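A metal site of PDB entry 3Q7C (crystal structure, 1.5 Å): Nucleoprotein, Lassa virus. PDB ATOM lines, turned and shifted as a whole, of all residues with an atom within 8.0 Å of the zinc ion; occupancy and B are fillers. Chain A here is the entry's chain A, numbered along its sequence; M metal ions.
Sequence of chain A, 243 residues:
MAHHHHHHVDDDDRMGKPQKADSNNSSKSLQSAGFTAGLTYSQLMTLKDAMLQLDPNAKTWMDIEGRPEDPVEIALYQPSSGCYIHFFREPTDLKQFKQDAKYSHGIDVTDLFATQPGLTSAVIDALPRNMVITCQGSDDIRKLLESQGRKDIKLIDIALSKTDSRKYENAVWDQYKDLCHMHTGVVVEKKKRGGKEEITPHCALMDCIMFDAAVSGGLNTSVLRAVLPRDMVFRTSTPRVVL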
ATOM      1  N   GLU A  65       5.967 -17.457 -25.966  1.00  0.00           N
ATOM      2  CA  GLU A  65       5.997 -18.163 -27.229  1.00  0.00           C
ATOM      3  C   GLU A  65       4.601 -18.125 -27.819  1.00  0.00           C
ATOM      4  O   GLU A  65       3.596 -18.175 -27.095  1.00  0.00           O
ATOM      5  CB  GLU A  65       6.478 -19.607 -27.048  1.00  0.00           C
ATOM      6  CG  GLU A  65       7.874 -19.733 -26.493  1.00  0.00           C
ATOM      7  CD  GLU A  65       8.922 -19.016 -27.318  1.00  0.00           C
ATOM      8  OE1 GLU A  65       8.815 -19.025 -28.553  1.00  0.00           O
ATOM      9  OE2 GLU A  65       9.855 -18.460 -26.704  1.00  0.00           O
ATOM     10  N   GLU A  73       2.734 -20.014 -24.472  1.00  0.00           N
ATOM     11  CA  GLU A  73       3.582 -20.184 -23.295  1.00  0.00           C
ATOM     12  C   GLU A  73       4.003 -18.820 -22.801  1.00  0.00           C
ATOM     13  O   GLU A  73       4.411 -17.984 -23.598  1.00  0.00           O
ATOM     14  CB  GLU A  73       4.827 -21.048 -23.639  1.00  0.00           C
ATOM     15  CG  GLU A  73       5.655 -21.364 -22.395  1.00  0.00           C
ATOM     16  CD  GLU A  73       6.944 -22.122 -22.717  1.00  0.00           C
ATOM     17  OE1 GLU A  73       7.549 -21.869 -23.774  1.00  0.00           O
ATOM     18  OE2 GLU A  73       7.354 -22.969 -21.872  1.00  0.00           O
ATOM     19  N   ILE A  74       3.827 -18.576 -21.505  1.00  0.00           N
ATOM     20  CA  ILE A  74       4.185 -17.287 -20.909  1.00  0.00           C
ATOM     21  C   ILE A  74       5.057 -17.532 -19.703  1.00  0.00           C
ATOM     22  O   ILE A  74       4.832 -18.472 -18.928  1.00  0.00           O
ATOM     23  CB  ILE A  74       2.922 -16.505 -20.502  1.00  0.00           C
ATOM     24  CG1 ILE A  74       2.128 -16.156 -21.771  1.00  0.00           C
ATOM     25  CG2 ILE A  74       3.275 -15.218 -19.777  1.00  0.00           C
ATOM     26  CD1 ILE A  74       0.851 -15.359 -21.526  1.00  0.00           C
ATOM     27  N   ALA A  75       6.107 -16.722 -19.564  1.00  0.00           N
ATOM     28  CA  ALA A  75       6.938 -16.781 -18.366  1.00  0.00           C
ATOM     29  C   ALA A  75       7.282 -15.394 -17.861  1.00  0.00           C
ATOM     30  O   ALA A  75       7.470 -14.472 -18.658  1.00  0.00           O
ATOM     31  CB  ALA A  75       8.218 -17.563 -18.627  1.00  0.00           C
ATOM     32  N   HIS A  86       5.102 -19.411 -14.825  1.00  0.00           N
ATOM     33  CA  HIS A  86       5.239 -20.142 -16.067  1.00  0.00           C
ATOM     34  C   HIS A  86       3.973 -20.933 -16.294  1.00  0.00           C
ATOM     35  O   HIS A  86       3.563 -21.743 -15.459  1.00  0.00           O
ATOM     36  CB  HIS A  86       6.451 -21.073 -15.961  1.00  0.00           C
ATOM     37  CG  HIS A  86       6.721 -21.880 -17.191  1.00  0.00           C
ATOM     38  ND1 HIS A  86       7.105 -23.205 -17.135  1.00  0.00           N
ATOM     39  CD2 HIS A  86       6.659 -21.562 -18.509  1.00  0.00           C
ATOM     40  CE1 HIS A  86       7.261 -23.661 -18.373  1.00  0.00           C
ATOM     41  NE2 HIS A  86       7.002 -22.682 -19.214  1.00  0.00           N
ATOM     42  N   PHE A  87       3.333 -20.676 -17.424  1.00  0.00           N
ATOM     43  CA  PHE A  87       2.111 -21.384 -17.763  1.00  0.00           C
ATOM     44  C   PHE A  87       1.853 -21.411 -19.261  1.00  0.00           C
ATOM     45  O   PHE A  87       2.600 -20.812 -20.028  1.00  0.00           O
ATOM     46  CB  PHE A  87       0.910 -20.772 -17.002  1.00  0.00           C
ATOM     47  CG  PHE A  87       0.633 -19.344 -17.356  1.00  0.00           C
ATOM     48  CD1 PHE A  87      -0.319 -19.042 -18.306  1.00  0.00           C
ATOM     49  CD2 PHE A  87       1.336 -18.307 -16.748  1.00  0.00           C
ATOM     50  CE1 PHE A  87      -0.574 -17.726 -18.652  1.00  0.00           C
ATOM     51  CE2 PHE A  87       1.090 -16.981 -17.095  1.00  0.00           C
ATOM     52  CZ  PHE A  87       0.119 -16.700 -18.043  1.00  0.00           C
ATOM     53  N   PHE A  88       0.782 -22.098 -19.655  1.00  0.00           N
ATOM     54  CA  PHE A  88       0.490 -22.404 -21.048  1.00  0.00           C
ATOM     55  C   PHE A  88      -0.949 -22.106 -21.379  1.00  0.00           C
ATOM     56  O   PHE A  88      -1.795 -21.949 -20.482  1.00  0.00           O
ATOM     57  CB  PHE A  88       0.788 -23.893 -21.317  1.00  0.00           C
ATOM     58  CG  PHE A  88       2.222 -24.259 -21.147  1.00  0.00           C
ATOM     59  CD1 PHE A  88       3.082 -24.250 -22.238  1.00  0.00           C
ATOM     60  CD2 PHE A  88       2.723 -24.620 -19.919  1.00  0.00           C
ATOM     61  CE1 PHE A  88       4.433 -24.594 -22.088  1.00  0.00           C
ATOM     62  CE2 PHE A  88       4.077 -24.955 -19.748  1.00  0.00           C
ATOM     63  CZ  PHE A  88       4.912 -24.944 -20.842  1.00  0.00           C
ATOM     64  N   HIS A 105       8.976 -23.235 -31.304  1.00  0.00           N
ATOM     65  CA  HIS A 105       8.842 -23.774 -29.950  1.00  0.00           C
ATOM     66  C   HIS A 105       8.702 -25.282 -29.801  1.00  0.00           C
ATOM     67  O   HIS A 105       8.892 -25.801 -28.717  1.00  0.00           O
ATOM     68  CB  HIS A 105       7.752 -23.038 -29.151  1.00  0.00           C
ATOM     69  CG  HIS A 105       6.392 -23.065 -29.791  1.00  0.00           C
ATOM     70  ND1 HIS A 105       5.720 -24.236 -30.062  1.00  0.00           N
ATOM     71  CD2 HIS A 105       5.580 -22.058 -30.176  1.00  0.00           C
ATOM     72  CE1 HIS A 105       4.546 -23.954 -30.603  1.00  0.00           C
ATOM     73  NE2 HIS A 105       4.425 -22.633 -30.663  1.00  0.00           N
ATOM     74  N   ILE A 107       6.232 -27.151 -29.377  1.00  0.00           N
ATOM     75  CA  ILE A 107       5.198 -27.658 -28.480  1.00  0.00           C
ATOM     76  C   ILE A 107       4.140 -28.466 -29.241  1.00  0.00           C
ATOM     77  O   ILE A 107       3.742 -28.067 -30.323  1.00  0.00           O
ATOM     78  CB  ILE A 107       4.519 -26.494 -27.720  1.00  0.00           C
ATOM     79  CG1 ILE A 107       5.568 -25.728 -26.909  1.00  0.00           C
ATOM     80  CG2 ILE A 107       3.404 -27.059 -26.805  1.00  0.00           C
ATOM     81  CD1 ILE A 107       5.064 -24.404 -26.312  1.00  0.00           C
ATOM     82  N   TRP A 173      19.725 -24.569 -20.458  1.00  0.00           N
ATOM     83  CA  TRP A 173      19.013 -25.836 -20.621  1.00  0.00           C
ATOM     84  C   TRP A 173      19.636 -26.934 -19.775  1.00  0.00           C
ATOM     85  O   TRP A 173      18.926 -27.762 -19.188  1.00  0.00           O
ATOM     86  CB  TRP A 173      18.952 -26.266 -22.079  1.00  0.00           C
ATOM     87  CG  TRP A 173      17.883 -25.576 -22.900  1.00  0.00           C
ATOM     88  CD1 TRP A 173      18.082 -24.561 -23.799  1.00  0.00           C
ATOM     89  CD2 TRP A 173      16.468 -25.850 -22.909  1.00  0.00           C
ATOM     90  NE1 TRP A 173      16.880 -24.191 -24.366  1.00  0.00           N
ATOM     91  CE2 TRP A 173      15.880 -24.969 -23.835  1.00  0.00           C
ATOM     92  CE3 TRP A 173      15.649 -26.741 -22.205  1.00  0.00           C
ATOM     93  CZ2 TRP A 173      14.494 -24.963 -24.087  1.00  0.00           C
ATOM     94  CZ3 TRP A 173      14.276 -26.737 -22.462  1.00  0.00           C
ATOM     95  CH2 TRP A 173      13.717 -25.855 -23.393  1.00  0.00           C
ATOM     96  N   LYS A 177      16.595 -27.654 -17.504  1.00  0.00           N
ATOM     97  CA  LYS A 177      15.687 -28.372 -18.404  1.00  0.00           C
ATOM     98  C   LYS A 177      14.507 -29.022 -17.675  1.00  0.00           C
ATOM     99  O   LYS A 177      13.433 -29.150 -18.249  1.00  0.00           O
ATOM    100  CB  LYS A 177      16.436 -29.398 -19.240  1.00  0.00           C
ATOM    101  CG  LYS A 177      17.219 -30.414 -18.438  1.00  0.00           C
ATOM    102  CD  LYS A 177      18.015 -31.328 -19.355  1.00  0.00           C
ATOM    103  CE  LYS A 177      19.008 -32.161 -18.558  1.00  0.00           C
ATOM    104  NZ  LYS A 177      18.348 -32.885 -17.436  1.00  0.00           N
ATOM    105  N   LEU A 179      12.666 -27.852 -15.573  1.00  0.00           N
ATOM    106  CA  LEU A 179      11.585 -26.881 -15.363  1.00  0.00           C
ATOM    107  C   LEU A 179      10.634 -26.753 -16.542  1.00  0.00           C
ATOM    108  O   LEU A 179       9.590 -26.142 -16.423  1.00  0.00           O
ATOM    109  CB  LEU A 179      12.137 -25.513 -15.016  1.00  0.00           C
ATOM    110  CG  LEU A 179      13.033 -25.484 -13.778  1.00  0.00           C
ATOM    111  CD1 LEU A 179      13.363 -24.043 -13.414  1.00  0.00           C
ATOM    112  CD2 LEU A 179      12.352 -26.205 -12.615  1.00  0.00           C
ATOM    113  N   CYS A 180      10.987 -27.315 -17.699  1.00  0.00           N
ATOM    114  CA  CYS A 180      10.034 -27.309 -18.798  1.00  0.00           C
ATOM    115  C   CYS A 180      10.277 -28.459 -19.739  1.00  0.00           C
ATOM    116  O   CYS A 180      11.274 -28.488 -20.485  1.00  0.00           O
ATOM    117  CB  CYS A 180      10.049 -25.990 -19.581  1.00  0.00           C
ATOM    118  SG  CYS A 180       8.625 -25.906 -20.716  1.00  0.00           S
ATOM    119  N   HIS A 181       9.326 -29.386 -19.711  1.00  0.00           N
ATOM    120  CA  HIS A 181       9.392 -30.589 -20.550  1.00  0.00           C
ATOM    121  C   HIS A 181       8.488 -30.516 -21.779  1.00  0.00           C
ATOM    122  O   HIS A 181       8.233 -31.524 -22.429  1.00  0.00           O
ATOM    123  CB  HIS A 181       9.013 -31.822 -19.722  1.00  0.00           C
ATOM    124  CG  HIS A 181       9.957 -32.120 -18.615  1.00  0.00           C
ATOM    125  ND1 HIS A 181      11.167 -32.760 -18.807  1.00  0.00           N
ATOM    126  CD2 HIS A 181       9.875 -31.880 -17.280  1.00  0.00           C
ATOM    127  CE1 HIS A 181      11.781 -32.897 -17.644  1.00  0.00           C
ATOM    128  NE2 HIS A 181      11.019 -32.376 -16.703  1.00  0.00           N
ATOM    129  N   MET A 182       7.994 -29.319 -22.103  1.00  0.00           N
ATOM    130  CA  MET A 182       6.951 -29.187 -23.103  1.00  0.00           C
ATOM    131  C   MET A 182       7.422 -29.064 -24.553  1.00  0.00           C
ATOM    132  O   MET A 182       6.605 -29.083 -25.477  1.00  0.00           O
ATOM    133  CB  MET A 182       6.035 -28.007 -22.743  1.00  0.00           C
ATOM    134  CG  MET A 182       5.213 -28.265 -21.467  1.00  0.00           C
ATOM    135  SD  MET A 182       3.787 -29.315 -21.721  1.00  0.00           S
ATOM    136  CE  MET A 182       2.658 -28.139 -22.519  1.00  0.00           C
ATOM    137  N   HIS A 183       8.728 -28.954 -24.777  1.00  0.00           N
ATOM    138  CA  HIS A 183       9.234 -28.727 -26.120  1.00  0.00           C
ATOM    139  C   HIS A 183       9.703 -30.030 -26.716  1.00  0.00           C
ATOM    140  O   HIS A 183      10.892 -30.347 -26.679  1.00  0.00           O
ATOM    141  CB  HIS A 183      10.312 -27.651 -26.098  1.00  0.00           C
ATOM    142  CG  HIS A 183       9.834 -26.425 -25.402  1.00  0.00           C
ATOM    143  ND1 HIS A 183       9.228 -25.380 -26.064  1.00  0.00           N
ATOM    144  CD2 HIS A 183       9.772 -26.119 -24.085  1.00  0.00           C
ATOM    145  CE1 HIS A 183       8.852 -24.468 -25.187  1.00  0.00           C
ATOM    146  NE2 HIS A 183       9.168 -24.896 -23.977  1.00  0.00           N
ATOM    147  N   PRO A 201      14.814 -25.698 -29.372  1.00  0.00           N
ATOM    148  CA  PRO A 201      13.515 -25.021 -29.288  1.00  0.00           C
ATOM    149  C   PRO A 201      13.562 -23.805 -28.376  1.00  0.00           C
ATOM    150  O   PRO A 201      14.433 -23.714 -27.483  1.00  0.00           O
ATOM    151  CB  PRO A 201      12.605 -26.095 -28.682  1.00  0.00           C
ATOM    152  CG  PRO A 201      13.532 -26.987 -27.925  1.00  0.00           C
ATOM    153  CD  PRO A 201      14.796 -27.042 -28.765  1.00  0.00           C
ATOM    154  N   HIS A 202      12.654 -22.871 -28.627  1.00  0.00           N
ATOM    155  CA  HIS A 202      12.520 -21.678 -27.815  1.00  0.00           C
ATOM    156  C   HIS A 202      11.443 -21.886 -26.745  1.00  0.00           C
ATOM    157  O   HIS A 202      10.308 -22.263 -27.056  1.00  0.00           O
ATOM    158  CB  HIS A 202      12.176 -20.478 -28.689  1.00  0.00           C
ATOM    159  CG  HIS A 202      13.235 -20.145 -29.690  1.00  0.00           C
ATOM    160  ND1 HIS A 202      13.029 -19.269 -30.724  1.00  0.00           N
ATOM    161  CD2 HIS A 202      14.516 -20.565 -29.792  1.00  0.00           C
ATOM    162  CE1 HIS A 202      14.136 -19.176 -31.446  1.00  0.00           C
ATOM    163  NE2 HIS A 202      15.054 -19.949 -30.899  1.00  0.00           N
ATOM    164  N   CYS A 203      11.856 -21.671 -25.504  1.00  0.00           N
ATOM    165  CA  CYS A 203      10.998 -21.795 -24.328  1.00  0.00           C
ATOM    166  C   CYS A 203      10.939 -20.428 -23.662  1.00  0.00           C
ATOM    167  O   CYS A 203      11.967 -19.770 -23.461  1.00  0.00           O
ATOM    168  CB  CYS A 203      11.630 -22.805 -23.375  1.00  0.00           C
ATOM    169  SG  CYS A 203      10.896 -22.849 -21.718  1.00  0.00           S
ATOM    170  N   ALA A 204       9.729 -19.981 -23.320  1.00  0.00           N
ATOM    171  CA  ALA A 204       9.590 -18.662 -22.711  1.00  0.00           C
ATOM    172  C   ALA A 204      10.362 -18.564 -21.387  1.00  0.00           C
ATOM    173  O   ALA A 204      10.907 -17.511 -21.057  1.00  0.00           O
ATOM    174  CB  ALA A 204       8.119 -18.339 -22.500  1.00  0.00           C
ATOM    175  N   LEU A 205      10.366 -19.648 -20.623  1.00  0.00           N
ATOM    176  CA  LEU A 205      11.048 -19.634 -19.329  1.00  0.00           C
ATOM    177  C   LEU A 205      12.576 -19.655 -19.495  1.00  0.00           C
ATOM    178  O   LEU A 205      13.279 -18.827 -18.907  1.00  0.00           O
ATOM    179  CB  LEU A 205      10.600 -20.793 -18.456  1.00  0.00           C
ATOM    180  CG  LEU A 205      11.276 -20.908 -17.089  1.00  0.00           C
ATOM    181  CD1 LEU A 205      11.076 -19.654 -16.236  1.00  0.00           C
ATOM    182  CD2 LEU A 205      10.718 -22.146 -16.364  1.00  0.00           C
ATOM    183  N   MET A 206      13.072 -20.554 -20.334  1.00  0.00           N
ATOM    184  CA  MET A 206      14.522 -20.582 -20.584  1.00  0.00           C
ATOM    185  C   MET A 206      14.988 -19.281 -21.207  1.00  0.00           C
ATOM    186  O   MET A 206      16.104 -18.843 -20.930  1.00  0.00           O
ATOM    187  CB  MET A 206      14.955 -21.760 -21.473  1.00  0.00           C
ATOM    188  CG  MET A 206      14.504 -23.123 -20.968  1.00  0.00           C
ATOM    189  SD  MET A 206      15.062 -23.509 -19.296  1.00  0.00           S
ATOM    190  CE  MET A 206      13.732 -24.562 -18.747  1.00  0.00           C
ATOM    191  N   ASP A 207      14.154 -18.667 -22.050  1.00  0.00           N
ATOM    192  CA  ASP A 207      14.491 -17.369 -22.591  1.00  0.00           C
ATOM    193  C   ASP A 207      14.724 -16.335 -21.485  1.00  0.00           C
ATOM    194  O   ASP A 207      15.734 -15.643 -21.480  1.00  0.00           O
ATOM    195  CB  ASP A 207      13.399 -16.849 -23.520  1.00  0.00           C
ATOM    196  CG  ASP A 207      13.495 -17.410 -24.926  1.00  0.00           C
ATOM    197  OD1 ASP A 207      14.454 -18.117 -25.252  1.00  0.00           O
ATOM    198  OD2 ASP A 207      12.592 -17.117 -25.726  1.00  0.00           O
HETATM  199 ZN    ZN M   1       8.993 -24.087 -22.090  1.00  0.00          ZN
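The backbone carbonyl oxygen (O) of His 105 lies within hydrogen-bond range of a ring nitrogen (ND1) of His 183, 2.7 Å away. The side-chain sulfur of Cys 203 lies close to the backbone NH of Leu 205. OE1 of Glu 73 lies within hydrogen-bond range of N of Ala 204. O of Glu 73 is in hydrogen-bond range of N of Glu 65. The side-chain sulfur (SG) of Cys 203 sits close to the backbone NH (N) of Met 206 (3.5 Å). The backbone NH (N) of Met 182 sits close to the side-chain sulfur (SG) of Cys 180, 3.7 Å away. O of His 202 sits close to ND1 of His 183 (3.4 Å). The side-chain carboxylate (OE2) of Glu 73 sits close to a ring nitrogen (NE2) of His 86, 2.7 Å away.
NE2 of His 86 touches the zinc ion, at 3.8 Å. Within 4 Å of the zinc ion: Glu 73, His 86, Cys 180, His 183 and Cys 203.
OE2 of Glu 73 is bound to the zinc ion (2.0 Å). The zinc ion is bound by NE2 of His 183 (2.1 Å). The zinc ion is bound by SG of Cys 203 (2.3 Å). The side-chain sulfur (SG) of Cys 180 binds the zinc ion. The zinc ion has four donor atoms within binding distance.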
